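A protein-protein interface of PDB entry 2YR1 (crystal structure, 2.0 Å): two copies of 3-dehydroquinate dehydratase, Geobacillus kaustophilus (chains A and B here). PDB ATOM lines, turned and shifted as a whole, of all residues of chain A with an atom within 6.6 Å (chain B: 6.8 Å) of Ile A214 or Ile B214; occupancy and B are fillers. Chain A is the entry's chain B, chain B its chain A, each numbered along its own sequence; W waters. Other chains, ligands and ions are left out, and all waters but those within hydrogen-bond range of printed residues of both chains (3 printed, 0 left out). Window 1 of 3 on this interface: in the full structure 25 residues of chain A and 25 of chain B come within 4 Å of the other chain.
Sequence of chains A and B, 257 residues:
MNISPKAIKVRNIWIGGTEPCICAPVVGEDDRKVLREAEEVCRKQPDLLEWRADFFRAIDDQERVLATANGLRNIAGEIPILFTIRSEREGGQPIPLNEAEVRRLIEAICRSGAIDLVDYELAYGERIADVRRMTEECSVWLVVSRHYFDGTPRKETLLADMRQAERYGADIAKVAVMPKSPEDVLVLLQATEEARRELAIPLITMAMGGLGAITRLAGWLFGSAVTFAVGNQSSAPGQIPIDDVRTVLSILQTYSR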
ATOM      1  N   VAL A 185     -22.638   9.487 -16.859  1.00  0.00           N
ATOM      2  CA  VAL A 185     -22.187   8.853 -15.625  1.00  0.00           C
ATOM      3  C   VAL A 185     -21.010   7.930 -15.924  1.00  0.00           C
ATOM      4  O   VAL A 185     -20.052   7.860 -15.154  1.00  0.00           O
ATOM      5  CB  VAL A 185     -23.306   8.033 -14.941  1.00  0.00           C
ATOM      6  CG1 VAL A 185     -22.721   7.271 -13.710  1.00  0.00           C
ATOM      7  CG2 VAL A 185     -24.447   8.952 -14.495  1.00  0.00           C
ATOM      8  N   LEU A 189     -16.962   7.949 -14.635  1.00  0.00           N
ATOM      9  CA  LEU A 189     -16.275   6.771 -14.101  1.00  0.00           C
ATOM     10  C   LEU A 189     -15.043   6.378 -14.938  1.00  0.00           C
ATOM     11  O   LEU A 189     -14.002   5.981 -14.392  1.00  0.00           O
ATOM     12  CB  LEU A 189     -17.241   5.575 -13.999  1.00  0.00           C
ATOM     13  CG  LEU A 189     -18.367   5.809 -12.979  1.00  0.00           C
ATOM     14  CD1 LEU A 189     -19.325   4.638 -12.943  1.00  0.00           C
ATOM     15  CD2 LEU A 189     -17.739   6.031 -11.597  1.00  0.00           C
ATOM     16  N   ALA A 207     -20.499  12.307  -9.931  1.00  0.00           N
ATOM     17  CA  ALA A 207     -21.476  12.806 -10.899  1.00  0.00           C
ATOM     18  C   ALA A 207     -22.587  13.215  -9.941  1.00  0.00           C
ATOM     19  O   ALA A 207     -23.018  12.415  -9.104  1.00  0.00           O
ATOM     20  CB  ALA A 207     -21.948  11.714 -11.813  1.00  0.00           C
ATOM     21  N   GLY A 209     -26.444  14.970  -8.727  1.00  0.00           N
ATOM     22  CA  GLY A 209     -27.835  14.639  -8.997  1.00  0.00           C
ATOM     23  C   GLY A 209     -28.204  13.169  -8.845  1.00  0.00           C
ATOM     24  O   GLY A 209     -27.376  12.339  -8.427  1.00  0.00           O
ATOM     25  N   GLY A 210     -29.462  12.854  -9.189  1.00  0.00           N
ATOM     26  CA  GLY A 210     -29.962  11.492  -9.092  1.00  0.00           C
ATOM     27  C   GLY A 210     -29.199  10.470  -9.929  1.00  0.00           C
ATOM     28  O   GLY A 210     -28.778   9.433  -9.415  1.00  0.00           O
ATOM     29  N   LEU A 211     -29.004  10.765 -11.212  1.00  0.00           N
ATOM     30  CA  LEU A 211     -28.288   9.864 -12.120  1.00  0.00           C
ATOM     31  C   LEU A 211     -26.892   9.504 -11.605  1.00  0.00           C
ATOM     32  O   LEU A 211     -26.394   8.409 -11.862  1.00  0.00           O
ATOM     33  CB  LEU A 211     -28.115  10.505 -13.497  1.00  0.00           C
ATOM     34  CG  LEU A 211     -29.170  10.426 -14.597  1.00  0.00           C
ATOM     35  CD1 LEU A 211     -28.656  11.231 -15.796  1.00  0.00           C
ATOM     36  CD2 LEU A 211     -29.431   8.963 -14.988  1.00  0.00           C
ATOM     37  N   GLY A 212     -26.265  10.435 -10.890  1.00  0.00           N
ATOM     38  CA  GLY A 212     -24.922  10.185 -10.376  1.00  0.00           C
ATOM     39  C   GLY A 212     -24.837   9.481  -9.027  1.00  0.00           C
ATOM     40  O   GLY A 212     -23.734   9.284  -8.491  1.00  0.00           O
ATOM     41  N   ALA A 213     -25.973   9.060  -8.484  1.00  0.00           N
ATOM     42  CA  ALA A 213     -25.953   8.417  -7.167  1.00  0.00           C
ATOM     43  C   ALA A 213     -24.973   7.251  -7.120  1.00  0.00           C
ATOM     44  O   ALA A 213     -24.223   7.079  -6.142  1.00  0.00           O
ATOM     45  CB  ALA A 213     -27.370   7.951  -6.769  1.00  0.00           C
ATOM     46  N   ILE A 214     -24.922   6.473  -8.200  1.00  0.00           N
ATOM     47  CA  ILE A 214     -24.031   5.326  -8.215  1.00  0.00           C
ATOM     48  C   ILE A 214     -22.547   5.697  -8.083  1.00  0.00           C
ATOM     49  O   ILE A 214     -21.756   4.879  -7.593  1.00  0.00           O
ATOM     50  CB  ILE A 214     -24.246   4.457  -9.504  1.00  0.00           C
ATOM     51  CG1 ILE A 214     -23.383   3.197  -9.436  1.00  0.00           C
ATOM     52  CG2 ILE A 214     -23.897   5.257 -10.733  1.00  0.00           C
ATOM     53  CD1 ILE A 214     -23.720   2.288  -8.235  1.00  0.00           C
ATOM     54  N   THR A 215     -22.168   6.903  -8.517  1.00  0.00           N
ATOM     55  CA  THR A 215     -20.772   7.334  -8.422  1.00  0.00           C
ATOM     56  C   THR A 215     -20.421   7.666  -6.996  1.00  0.00           C
ATOM     57  O   THR A 215     -19.255   7.571  -6.609  1.00  0.00           O
ATOM     58  CB  THR A 215     -20.428   8.564  -9.338  1.00  0.00           C
ATOM     59  OG1 THR A 215     -21.032   9.771  -8.829  1.00  0.00           O
ATOM     60  CG2 THR A 215     -20.932   8.304 -10.752  1.00  0.00           C
ATOM     61  N   ARG A 216     -21.410   8.045  -6.190  1.00  0.00           N
ATOM     62  CA  ARG A 216     -21.107   8.338  -4.789  1.00  0.00           C
ATOM     63  C   ARG A 216     -20.979   7.032  -3.981  1.00  0.00           C
ATOM     64  O   ARG A 216     -20.264   6.970  -2.974  1.00  0.00           O
ATOM     65  CB  ARG A 216     -22.181   9.227  -4.170  1.00  0.00           C
ATOM     66  CG  ARG A 216     -22.348  10.571  -4.886  1.00  0.00           C
ATOM     67  CD  ARG A 216     -23.318  11.443  -4.141  1.00  0.00           C
ATOM     68  NE  ARG A 216     -23.557  12.715  -4.805  1.00  0.00           N
ATOM     69  CZ  ARG A 216     -22.759  13.769  -4.722  1.00  0.00           C
ATOM     70  NH1 ARG A 216     -21.640  13.714  -4.002  1.00  0.00           N
ATOM     71  NH2 ARG A 216     -23.108  14.894  -5.322  1.00  0.00           N
ATOM     72  N   LEU A 217     -21.631   5.976  -4.463  1.00  0.00           N
ATOM     73  CA  LEU A 217     -21.630   4.679  -3.774  1.00  0.00           C
ATOM     74  C   LEU A 217     -20.588   3.691  -4.283  1.00  0.00           C
ATOM     75  O   LEU A 217     -20.178   2.777  -3.557  1.00  0.00           O
ATOM     76  CB  LEU A 217     -23.015   4.036  -3.904  1.00  0.00           C
ATOM     77  CG  LEU A 217     -24.170   4.919  -3.424  1.00  0.00           C
ATOM     78  CD1 LEU A 217     -25.523   4.269  -3.708  1.00  0.00           C
ATOM     79  CD2 LEU A 217     -23.998   5.166  -1.956  1.00  0.00           C
ATOM     80  N   ALA A 218     -20.149   3.875  -5.523  1.00  0.00           N
ATOM     81  CA  ALA A 218     -19.197   2.950  -6.120  1.00  0.00           C
ATOM     82  C   ALA A 218     -18.035   3.583  -6.867  1.00  0.00           C
ATOM     83  O   ALA A 218     -17.263   2.886  -7.515  1.00  0.00           O
ATOM     84  CB  ALA A 218     -19.938   2.032  -7.043  1.00  0.00           C
ATOM     85  N   GLY A 219     -17.914   4.904  -6.819  1.00  0.00           N
ATOM     86  CA  GLY A 219     -16.808   5.516  -7.524  1.00  0.00           C
ATOM     87  C   GLY A 219     -15.451   5.028  -7.019  1.00  0.00           C
ATOM     88  O   GLY A 219     -14.464   5.030  -7.756  1.00  0.00           O
ATOM     89  N   LEU A 221     -14.468   2.123  -6.539  1.00  0.00           N
ATOM     90  CA  LEU A 221     -14.050   0.941  -7.279  1.00  0.00           C
ATOM     91  C   LEU A 221     -13.260   1.387  -8.509  1.00  0.00           C
ATOM     92  O   LEU A 221     -12.565   0.584  -9.136  1.00  0.00           O
ATOM     93  CB  LEU A 221     -15.278   0.132  -7.725  1.00  0.00           C
ATOM     94  CG  LEU A 221     -16.112  -0.523  -6.613  1.00  0.00           C
ATOM     95  CD1 LEU A 221     -17.420  -1.014  -7.196  1.00  0.00           C
ATOM     96  CD2 LEU A 221     -15.332  -1.687  -5.981  1.00  0.00           C
ATOM     97  N   PHE A 222     -13.376   2.664  -8.868  1.00  0.00           N
ATOM     98  CA  PHE A 222     -12.667   3.169 -10.043  1.00  0.00           C
ATOM     99  C   PHE A 222     -11.644   4.259  -9.732  1.00  0.00           C
ATOM    100  O   PHE A 222     -11.140   4.941 -10.626  1.00  0.00           O
ATOM    101  CB  PHE A 222     -13.697   3.644 -11.077  1.00  0.00           C
ATOM    102  CG  PHE A 222     -14.675   2.575 -11.456  1.00  0.00           C
ATOM    103  CD1 PHE A 222     -14.298   1.545 -12.314  1.00  0.00           C
ATOM    104  CD2 PHE A 222     -15.930   2.526 -10.874  1.00  0.00           C
ATOM    105  CE1 PHE A 222     -15.166   0.479 -12.578  1.00  0.00           C
ATOM    106  CE2 PHE A 222     -16.805   1.471 -11.126  1.00  0.00           C
ATOM    107  CZ  PHE A 222     -16.420   0.446 -11.979  1.00  0.00           C
ATOM    108  N   ILE A 240     -26.045  11.583  -0.596  1.00  0.00           N
ATOM    109  CA  ILE A 240     -26.880  10.622   0.102  1.00  0.00           C
ATOM    110  C   ILE A 240     -26.583  10.571   1.600  1.00  0.00           C
ATOM    111  O   ILE A 240     -25.432  10.695   2.006  1.00  0.00           O
ATOM    112  CB  ILE A 240     -26.625   9.225  -0.481  1.00  0.00           C
ATOM    113  CG1 ILE A 240     -26.817   9.271  -2.008  1.00  0.00           C
ATOM    114  CG2 ILE A 240     -27.545   8.204   0.183  1.00  0.00           C
ATOM    115  CD1 ILE A 240     -26.374   7.988  -2.717  1.00  0.00           C
ATOM    116  N   VAL A 248     -24.338   0.534   1.830  1.00  0.00           N
ATOM    117  CA  VAL A 248     -23.938   0.084   0.500  1.00  0.00           C
ATOM    118  C   VAL A 248     -22.434  -0.205   0.412  1.00  0.00           C
ATOM    119  O   VAL A 248     -22.031  -1.192  -0.203  1.00  0.00           O
ATOM    120  CB  VAL A 248     -24.349   1.123  -0.584  1.00  0.00           C
ATOM    121  CG1 VAL A 248     -23.775   0.727  -1.948  1.00  0.00           C
ATOM    122  CG2 VAL A 248     -25.880   1.203  -0.665  1.00  0.00           C
ATOM    123  N   LEU A 252     -20.749  -3.605  -0.826  1.00  0.00           N
ATOM    124  CA  LEU A 252     -19.860  -3.560  -1.984  1.00  0.00           C
ATOM    125  C   LEU A 252     -18.460  -4.096  -1.651  1.00  0.00           C
ATOM    126  O   LEU A 252     -17.869  -4.839  -2.428  1.00  0.00           O
ATOM    127  CB  LEU A 252     -19.766  -2.125  -2.495  1.00  0.00           C
ATOM    128  CG  LEU A 252     -19.547  -1.909  -3.991  1.00  0.00           C
ATOM    129  CD1 LEU A 252     -20.527  -2.751  -4.804  1.00  0.00           C
ATOM    130  CD2 LEU A 252     -19.715  -0.411  -4.296  1.00  0.00           C
ATOM    131  N   TYR A 255     -18.431  -8.001  -1.123  1.00  0.00           N
ATOM    132  CA  TYR A 255     -18.578  -8.739  -2.368  1.00  0.00           C
ATOM    133  C   TYR A 255     -17.749  -8.319  -3.567  1.00  0.00           C
ATOM    134  O   TYR A 255     -17.864  -8.930  -4.632  1.00  0.00           O
ATOM    135  CB  TYR A 255     -20.046  -8.769  -2.773  1.00  0.00           C
ATOM    136  CG  TYR A 255     -20.902  -9.509  -1.780  1.00  0.00           C
ATOM    137  CD1 TYR A 255     -20.700 -10.862  -1.538  1.00  0.00           C
ATOM    138  CD2 TYR A 255     -21.896  -8.848  -1.064  1.00  0.00           C
ATOM    139  CE1 TYR A 255     -21.469 -11.540  -0.598  1.00  0.00           C
ATOM    140  CE2 TYR A 255     -22.667  -9.514  -0.129  1.00  0.00           C
ATOM    141  CZ  TYR A 255     -22.450 -10.855   0.102  1.00  0.00           C
ATOM    142  OH  TYR A 255     -23.210 -11.512   1.038  1.00  0.00           O
ATOM    143  N   SER A 256     -16.923  -7.294  -3.413  1.00  0.00           N
ATOM    144  CA  SER A 256     -16.090  -6.853  -4.520  1.00  0.00           C
ATOM    145  C   SER A 256     -14.694  -7.433  -4.379  1.00  0.00           C
ATOM    146  O   SER A 256     -13.936  -7.051  -3.492  1.00  0.00           O
ATOM    147  CB  SER A 256     -16.030  -5.330  -4.583  1.00  0.00           C
ATOM    148  OG  SER A 256     -17.231  -4.818  -5.134  1.00  0.00           O
ATOM    149  N   VAL B 185     -14.950  -3.813 -16.457  1.00  0.00           N
ATOM    150  CA  VAL B 185     -16.284  -3.649 -15.890  1.00  0.00           C
ATOM    151  C   VAL B 185     -17.001  -2.489 -16.577  1.00  0.00           C
ATOM    152  O   VAL B 185     -18.168  -2.599 -16.923  1.00  0.00           O
ATOM    153  CB  VAL B 185     -16.214  -3.409 -14.357  1.00  0.00           C
ATOM    154  CG1 VAL B 185     -17.587  -3.183 -13.800  1.00  0.00           C
ATOM    155  CG2 VAL B 185     -15.574  -4.628 -13.677  1.00  0.00           C
ATOM    156  N   LEU B 186     -16.290  -1.390 -16.807  1.00  0.00           N
ATOM    157  CA  LEU B 186     -16.880  -0.229 -17.471  1.00  0.00           C
ATOM    158  C   LEU B 186     -17.187  -0.583 -18.949  1.00  0.00           C
ATOM    159  O   LEU B 186     -18.176  -0.129 -19.489  1.00  0.00           O
ATOM    160  CB  LEU B 186     -15.923   0.968 -17.360  1.00  0.00           C
ATOM    161  CG  LEU B 186     -15.691   1.485 -15.922  1.00  0.00           C
ATOM    162  CD1 LEU B 186     -14.785   2.703 -15.960  1.00  0.00           C
ATOM    163  CD2 LEU B 186     -17.030   1.853 -15.259  1.00  0.00           C
ATOM    164  N   LEU B 189     -20.525  -2.195 -18.993  1.00  0.00           N
ATOM    165  CA  LEU B 189     -21.632  -1.250 -18.775  1.00  0.00           C
ATOM    166  C   LEU B 189     -21.835  -0.373 -20.015  1.00  0.00           C
ATOM    167  O   LEU B 189     -22.966  -0.085 -20.415  1.00  0.00           O
ATOM    168  CB  LEU B 189     -21.350  -0.374 -17.547  1.00  0.00           C
ATOM    169  CG  LEU B 189     -21.284  -1.112 -16.204  1.00  0.00           C
ATOM    170  CD1 LEU B 189     -20.998  -0.117 -15.083  1.00  0.00           C
ATOM    171  CD2 LEU B 189     -22.594  -1.840 -15.946  1.00  0.00           C
ATOM    172  N   ALA B 207     -20.929  -8.619 -15.400  1.00  0.00           N
ATOM    173  CA  ALA B 207     -19.493  -8.889 -15.371  1.00  0.00           C
ATOM    174  C   ALA B 207     -19.516  -9.797 -14.136  1.00  0.00           C
ATOM    175  O   ALA B 207     -20.105  -9.440 -13.102  1.00  0.00           O
ATOM    176  CB  ALA B 207     -18.686  -7.618 -15.085  1.00  0.00           C
ATOM    177  N   GLY B 209     -17.609 -12.487 -11.169  1.00  0.00           N
ATOM    178  CA  GLY B 209     -16.538 -12.283 -10.208  1.00  0.00           C
ATOM    179  C   GLY B 209     -16.713 -11.102  -9.257  1.00  0.00           C
ATOM    180  O   GLY B 209     -17.699 -10.351  -9.340  1.00  0.00           O
ATOM    181  N   GLY B 210     -15.735 -10.918  -8.367  1.00  0.00           N
ATOM    182  CA  GLY B 210     -15.810  -9.846  -7.383  1.00  0.00           C
ATOM    183  C   GLY B 210     -15.781  -8.496  -8.068  1.00  0.00           C
ATOM    184  O   GLY B 210     -16.499  -7.564  -7.703  1.00  0.00           O
ATOM    185  N   LEU B 211     -14.929  -8.412  -9.075  1.00  0.00           N
ATOM    186  CA  LEU B 211     -14.759  -7.204  -9.862  1.00  0.00           C
ATOM    187  C   LEU B 211     -16.085  -6.770 -10.460  1.00  0.00           C
ATOM    188  O   LEU B 211     -16.369  -5.581 -10.546  1.00  0.00           O
ATOM    189  CB  LEU B 211     -13.763  -7.479 -10.979  1.00  0.00           C
ATOM    190  CG  LEU B 211     -12.582  -6.540 -11.186  1.00  0.00           C
ATOM    191  CD1 LEU B 211     -12.157  -5.895  -9.878  1.00  0.00           C
ATOM    192  CD2 LEU B 211     -11.458  -7.350 -11.806  1.00  0.00           C
ATOM    193  N   GLY B 212     -16.894  -7.740 -10.869  1.00  0.00           N
ATOM    194  CA  GLY B 212     -18.173  -7.429 -11.476  1.00  0.00           C
ATOM    195  C   GLY B 212     -19.371  -7.255 -10.556  1.00  0.00           C
ATOM    196  O   GLY B 212     -20.492  -7.054 -11.030  1.00  0.00           O
ATOM    197  N   ALA B 213     -19.154  -7.311  -9.247  1.00  0.00           N
ATOM    198  CA  ALA B 213     -20.267  -7.172  -8.324  1.00  0.00           C
ATOM    199  C   ALA B 213     -21.095  -5.922  -8.605  1.00  0.00           C
ATOM    200  O   ALA B 213     -22.328  -5.979  -8.620  1.00  0.00           O
ATOM    201  CB  ALA B 213     -19.763  -7.143  -6.881  1.00  0.00           C
ATOM    202  N   ILE B 214     -20.423  -4.798  -8.839  1.00  0.00           N
ATOM    203  CA  ILE B 214     -21.139  -3.546  -9.078  1.00  0.00           C
ATOM    204  C   ILE B 214     -22.160  -3.668 -10.189  1.00  0.00           C
ATOM    205  O   ILE B 214     -23.221  -3.025 -10.143  1.00  0.00           O
ATOM    206  CB  ILE B 214     -20.178  -2.354  -9.417  1.00  0.00           C
ATOM    207  CG1 ILE B 214     -20.976  -1.045  -9.494  1.00  0.00           C
ATOM    208  CG2 ILE B 214     -19.485  -2.584 -10.773  1.00  0.00           C
ATOM    209  CD1 ILE B 214     -21.677  -0.638  -8.177  1.00  0.00           C
ATOM    210  N   THR B 215     -21.847  -4.496 -11.180  1.00  0.00           N
ATOM    211  CA  THR B 215     -22.745  -4.665 -12.311  1.00  0.00           C
ATOM    212  C   THR B 215     -24.048  -5.382 -11.973  1.00  0.00           C
ATOM    213  O   THR B 215     -25.072  -5.167 -12.634  1.00  0.00           O
ATOM    214  CB  THR B 215     -22.023  -5.365 -13.466  1.00  0.00           C
ATOM    215  OG1 THR B 215     -22.631  -4.970 -14.689  1.00  0.00           O
ATOM    216  CG2 THR B 215     -22.105  -6.867 -13.342  1.00  0.00           C
ATOM    217  N   ARG B 216     -24.022  -6.215 -10.939  1.00  0.00           N
ATOM    218  CA  ARG B 216     -25.213  -6.937 -10.516  1.00  0.00           C
ATOM    219  C   ARG B 216     -26.120  -6.032  -9.681  1.00  0.00           C
ATOM    220  O   ARG B 216     -27.320  -6.274  -9.554  1.00  0.00           O
ATOM    221  CB  ARG B 216     -24.811  -8.181  -9.685  1.00  0.00           C
ATOM    222  CG  ARG B 216     -23.891  -9.140 -10.418  1.00  0.00           C
ATOM    223  CD  ARG B 216     -23.626 -10.408  -9.593  1.00  0.00           C
ATOM    224  NE  ARG B 216     -22.816 -11.402 -10.291  1.00  0.00           N
ATOM    225  CZ  ARG B 216     -23.258 -12.189 -11.270  1.00  0.00           C
ATOM    226  NH1 ARG B 216     -24.511 -12.105 -11.687  1.00  0.00           N
ATOM    227  NH2 ARG B 216     -22.449 -13.084 -11.825  1.00  0.00           N
ATOM    228  N   LEU B 217     -25.551  -4.972  -9.122  1.00  0.00           N
ATOM    229  CA  LEU B 217     -26.324  -4.070  -8.281  1.00  0.00           C
ATOM    230  C   LEU B 217     -26.728  -2.781  -8.992  1.00  0.00           C
ATOM    231  O   LEU B 217     -27.690  -2.135  -8.588  1.00  0.00           O
ATOM    232  CB  LEU B 217     -25.514  -3.707  -7.027  1.00  0.00           C
ATOM    233  CG  LEU B 217     -24.999  -4.823  -6.102  1.00  0.00           C
ATOM    234  CD1 LEU B 217     -24.025  -4.247  -5.100  1.00  0.00           C
ATOM    235  CD2 LEU B 217     -26.166  -5.500  -5.385  1.00  0.00           C
ATOM    236  N   ALA B 218     -25.992  -2.411 -10.041  1.00  0.00           N
ATOM    237  CA  ALA B 218     -26.262  -1.161 -10.748  1.00  0.00           C
ATOM    238  C   ALA B 218     -26.411  -1.271 -12.257  1.00  0.00           C
ATOM    239  O   ALA B 218     -26.595  -0.269 -12.931  1.00  0.00           O
ATOM    240  CB  ALA B 218     -25.157  -0.153 -10.425  1.00  0.00           C
ATOM    241  N   GLY B 219     -26.327  -2.477 -12.795  1.00  0.00           N
ATOM    242  CA  GLY B 219     -26.460  -2.620 -14.230  1.00  0.00           C
ATOM    243  C   GLY B 219     -27.796  -2.125 -14.753  1.00  0.00           C
ATOM    244  O   GLY B 219     -27.879  -1.652 -15.888  1.00  0.00           O
ATOM    245  N   LEU B 221     -29.209   0.482 -14.232  1.00  0.00           N
ATOM    246  CA  LEU B 221     -29.137   1.920 -14.531  1.00  0.00           C
ATOM    247  C   LEU B 221     -28.660   2.149 -15.977  1.00  0.00           C
ATOM    248  O   LEU B 221     -28.774   3.250 -16.531  1.00  0.00           O
ATOM    249  CB  LEU B 221     -28.153   2.609 -13.559  1.00  0.00           C
ATOM    250  CG  LEU B 221     -28.623   2.746 -12.097  1.00  0.00           C
ATOM    251  CD1 LEU B 221     -27.430   3.068 -11.190  1.00  0.00           C
ATOM    252  CD2 LEU B 221     -29.674   3.835 -11.980  1.00  0.00           C
ATOM    253  N   PHE B 222     -28.111   1.100 -16.574  1.00  0.00           N
ATOM    254  CA  PHE B 222     -27.566   1.170 -17.927  1.00  0.00           C
ATOM    255  C   PHE B 222     -28.294   0.261 -18.889  1.00  0.00           C
ATOM    256  O   PHE B 222     -27.871   0.094 -20.028  1.00  0.00           O
ATOM    257  CB  PHE B 222     -26.067   0.832 -17.895  1.00  0.00           C
ATOM    258  CG  PHE B 222     -25.288   1.730 -16.984  1.00  0.00           C
ATOM    259  CD1 PHE B 222     -24.976   3.032 -17.381  1.00  0.00           C
ATOM    260  CD2 PHE B 222     -24.966   1.321 -15.694  1.00  0.00           C
ATOM    261  CE1 PHE B 222     -24.361   3.919 -16.494  1.00  0.00           C
ATOM    262  CE2 PHE B 222     -24.356   2.191 -14.797  1.00  0.00           C
ATOM    263  CZ  PHE B 222     -24.053   3.501 -15.191  1.00  0.00           C
ATOM    264  N   ILE B 240     -24.365 -12.393  -5.585  1.00  0.00           N
ATOM    265  CA  ILE B 240     -24.556 -11.890  -4.226  1.00  0.00           C
ATOM    266  C   ILE B 240     -25.867 -12.374  -3.629  1.00  0.00           C
ATOM    267  O   ILE B 240     -26.844 -12.569  -4.350  1.00  0.00           O
ATOM    268  CB  ILE B 240     -24.584 -10.333  -4.239  1.00  0.00           C
ATOM    269  CG1 ILE B 240     -23.226  -9.801  -4.664  1.00  0.00           C
ATOM    270  CG2 ILE B 240     -24.989  -9.763  -2.894  1.00  0.00           C
ATOM    271  CD1 ILE B 240     -22.918 -10.057  -6.080  1.00  0.00           C
ATOM    272  N   VAL B 248     -29.303  -2.910  -1.401  1.00  0.00           N
ATOM    273  CA  VAL B 248     -28.675  -1.914  -2.278  1.00  0.00           C
ATOM    274  C   VAL B 248     -29.633  -1.346  -3.317  1.00  0.00           C
ATOM    275  O   VAL B 248     -29.658  -0.127  -3.572  1.00  0.00           O
ATOM    276  CB  VAL B 248     -27.427  -2.533  -2.979  1.00  0.00           C
ATOM    277  CG1 VAL B 248     -26.830  -1.566  -3.954  1.00  0.00           C
ATOM    278  CG2 VAL B 248     -26.392  -2.928  -1.911  1.00  0.00           C
ATOM    279  N   LEU B 252     -30.269   2.496  -3.832  1.00  0.00           N
ATOM    280  CA  LEU B 252     -29.928   3.030  -5.135  1.00  0.00           C
ATOM    281  C   LEU B 252     -31.171   3.588  -5.822  1.00  0.00           C
ATOM    282  O   LEU B 252     -31.107   4.636  -6.446  1.00  0.00           O
ATOM    283  CB  LEU B 252     -29.290   1.932  -5.994  1.00  0.00           C
ATOM    284  CG  LEU B 252     -28.475   2.345  -7.218  1.00  0.00           C
ATOM    285  CD1 LEU B 252     -27.419   3.398  -6.829  1.00  0.00           C
ATOM    286  CD2 LEU B 252     -27.819   1.089  -7.807  1.00  0.00           C
ATOM    287  N   SER B 256     -31.528   7.467  -6.855  1.00  0.00           N
ATOM    288  CA  SER B 256     -31.199   7.700  -8.266  1.00  0.00           C
ATOM    289  C   SER B 256     -32.289   8.513  -8.948  1.00  0.00           C
ATOM    290  O   SER B 256     -32.098   9.031 -10.051  1.00  0.00           O
ATOM    291  CB  SER B 256     -31.030   6.372  -9.017  1.00  0.00           C
ATOM    292  OG  SER B 256     -29.852   5.702  -8.611  1.00  0.00           O
HETATM  293  O   HOH W   1     -19.582 -10.201  -6.994  1.00  0.00           O
HETATM  294  O   HOH W   2     -27.282   6.364  -9.960  1.00  0.00           O
HETATM  295  O   HOH W   3     -17.765  -4.253  -8.005  1.00  0.00           O
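Among the printed residues, merely in contact across the chains: Ser A256 with Gly B210 (3.3 Å), Ala A218 with Ile B214 (3.4 Å), Tyr A255 with Ala B213 (3.4 Å), Phe A222 with Leu B186 (3.5 Å), Tyr A255 with Gly B210 (3.6 Å), Ile A214 with Ile B214 (3.6 Å), Ile A214 with Ala B218 (3.6 Å), Tyr A255 with Ile B240 (3.6 Å), Leu A189 with Leu B186 (3.7 Å), Leu A211 with Ser B256 (3.7 Å), Leu A217 with Leu B252 (3.8 Å), Leu A221 with Ile B214 (3.8 Å), Leu A252 with Leu B217 (3.8 Å), Ala A213 with Ser B256 (3.8 Å), Ser A256 with Ala B213 (3.9 Å) and Ile A214 with Leu B221 (3.9 Å).
Of the printed residues of chain B, Leu A189 touches Leu B186 (3.7 Å).
Ala A207 touches none of the printed residues of chain B.
Printed residues of chain B within 4 Å of Leu A211: Ser B256.
Of chain B, only Ile B214 (3.6 Å), Ala B218 (3.6 Å) and Leu B221 (3.9 Å) come within 4 Å of Ile A214.
Of the printed residues of chain A, Ile B214 touches Ile A214 (3.6 Å), Ala A218 (3.4 Å) and Leu A221 (3.8 Å).
Printed residues of chain A within 4 Å of Leu B252: Leu A217 (3.8 Å).
The side-chain hydroxyl of Ser B256 sits at hydrogen-bond distance from the backbone carbonyl oxygen of Leu B252, 2.7 Å away.
The side-chain hydroxyl of Ser A256 is in hydrogen-bond range of the backbone carbonyl oxygen of Leu A252, 2.8 Å away.
Water W3 lies within hydrogen-bond range of the backbone NH of Ile B214 (2.8 Å), the side-chain hydroxyl of Ser A256 (3.0 Å) and the backbone carbonyl oxygen of Leu B211 (3.2 Å).
Water W2 lies within hydrogen-bond range of the backbone carbonyl oxygen of Leu A211, the backbone NH of Ile A214, the side-chain hydroxyl of Ser B256, the backbone NH of Ala A213 and the backbone carbonyl oxygen of Gly A210.
Water W1 lies within hydrogen-bond range of O of Gly B209 (3.0 Å) and O of Tyr A255 (3.2 Å).
Hydrophobic or aromatic side chains of chain B that line the printed part of chain A: Leu B186, Ala B213, Ile B214, Leu B217, Ala B218, Leu B221, Ile B240 and Leu B252.
Among the printed residues, no Asp or Glu carboxylate lies within 4 Å of a Lys or Arg side-chain nitrogen of the other chain.
Gly A210 touches Ser B256, and with the chains exchanged Ser A256 touches Gly B210.
Ile B214 touches its own counterpart, Ile A214.
Ile A214 touches Leu B221, and with the chains exchanged Leu A221 touches Ile B214.
Leu A217 touches Leu B252, and with the chains exchanged Leu A252 touches Leu B217.
Of the 17 pairs that touch across the chains among the printed residues, 11 have their exchanged pair printed and touching as well.
The backbone carbonyl oxygen of Gly A210 lies close to the backbone carbonyl oxygen of Ser B256, 3.4 Å away.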
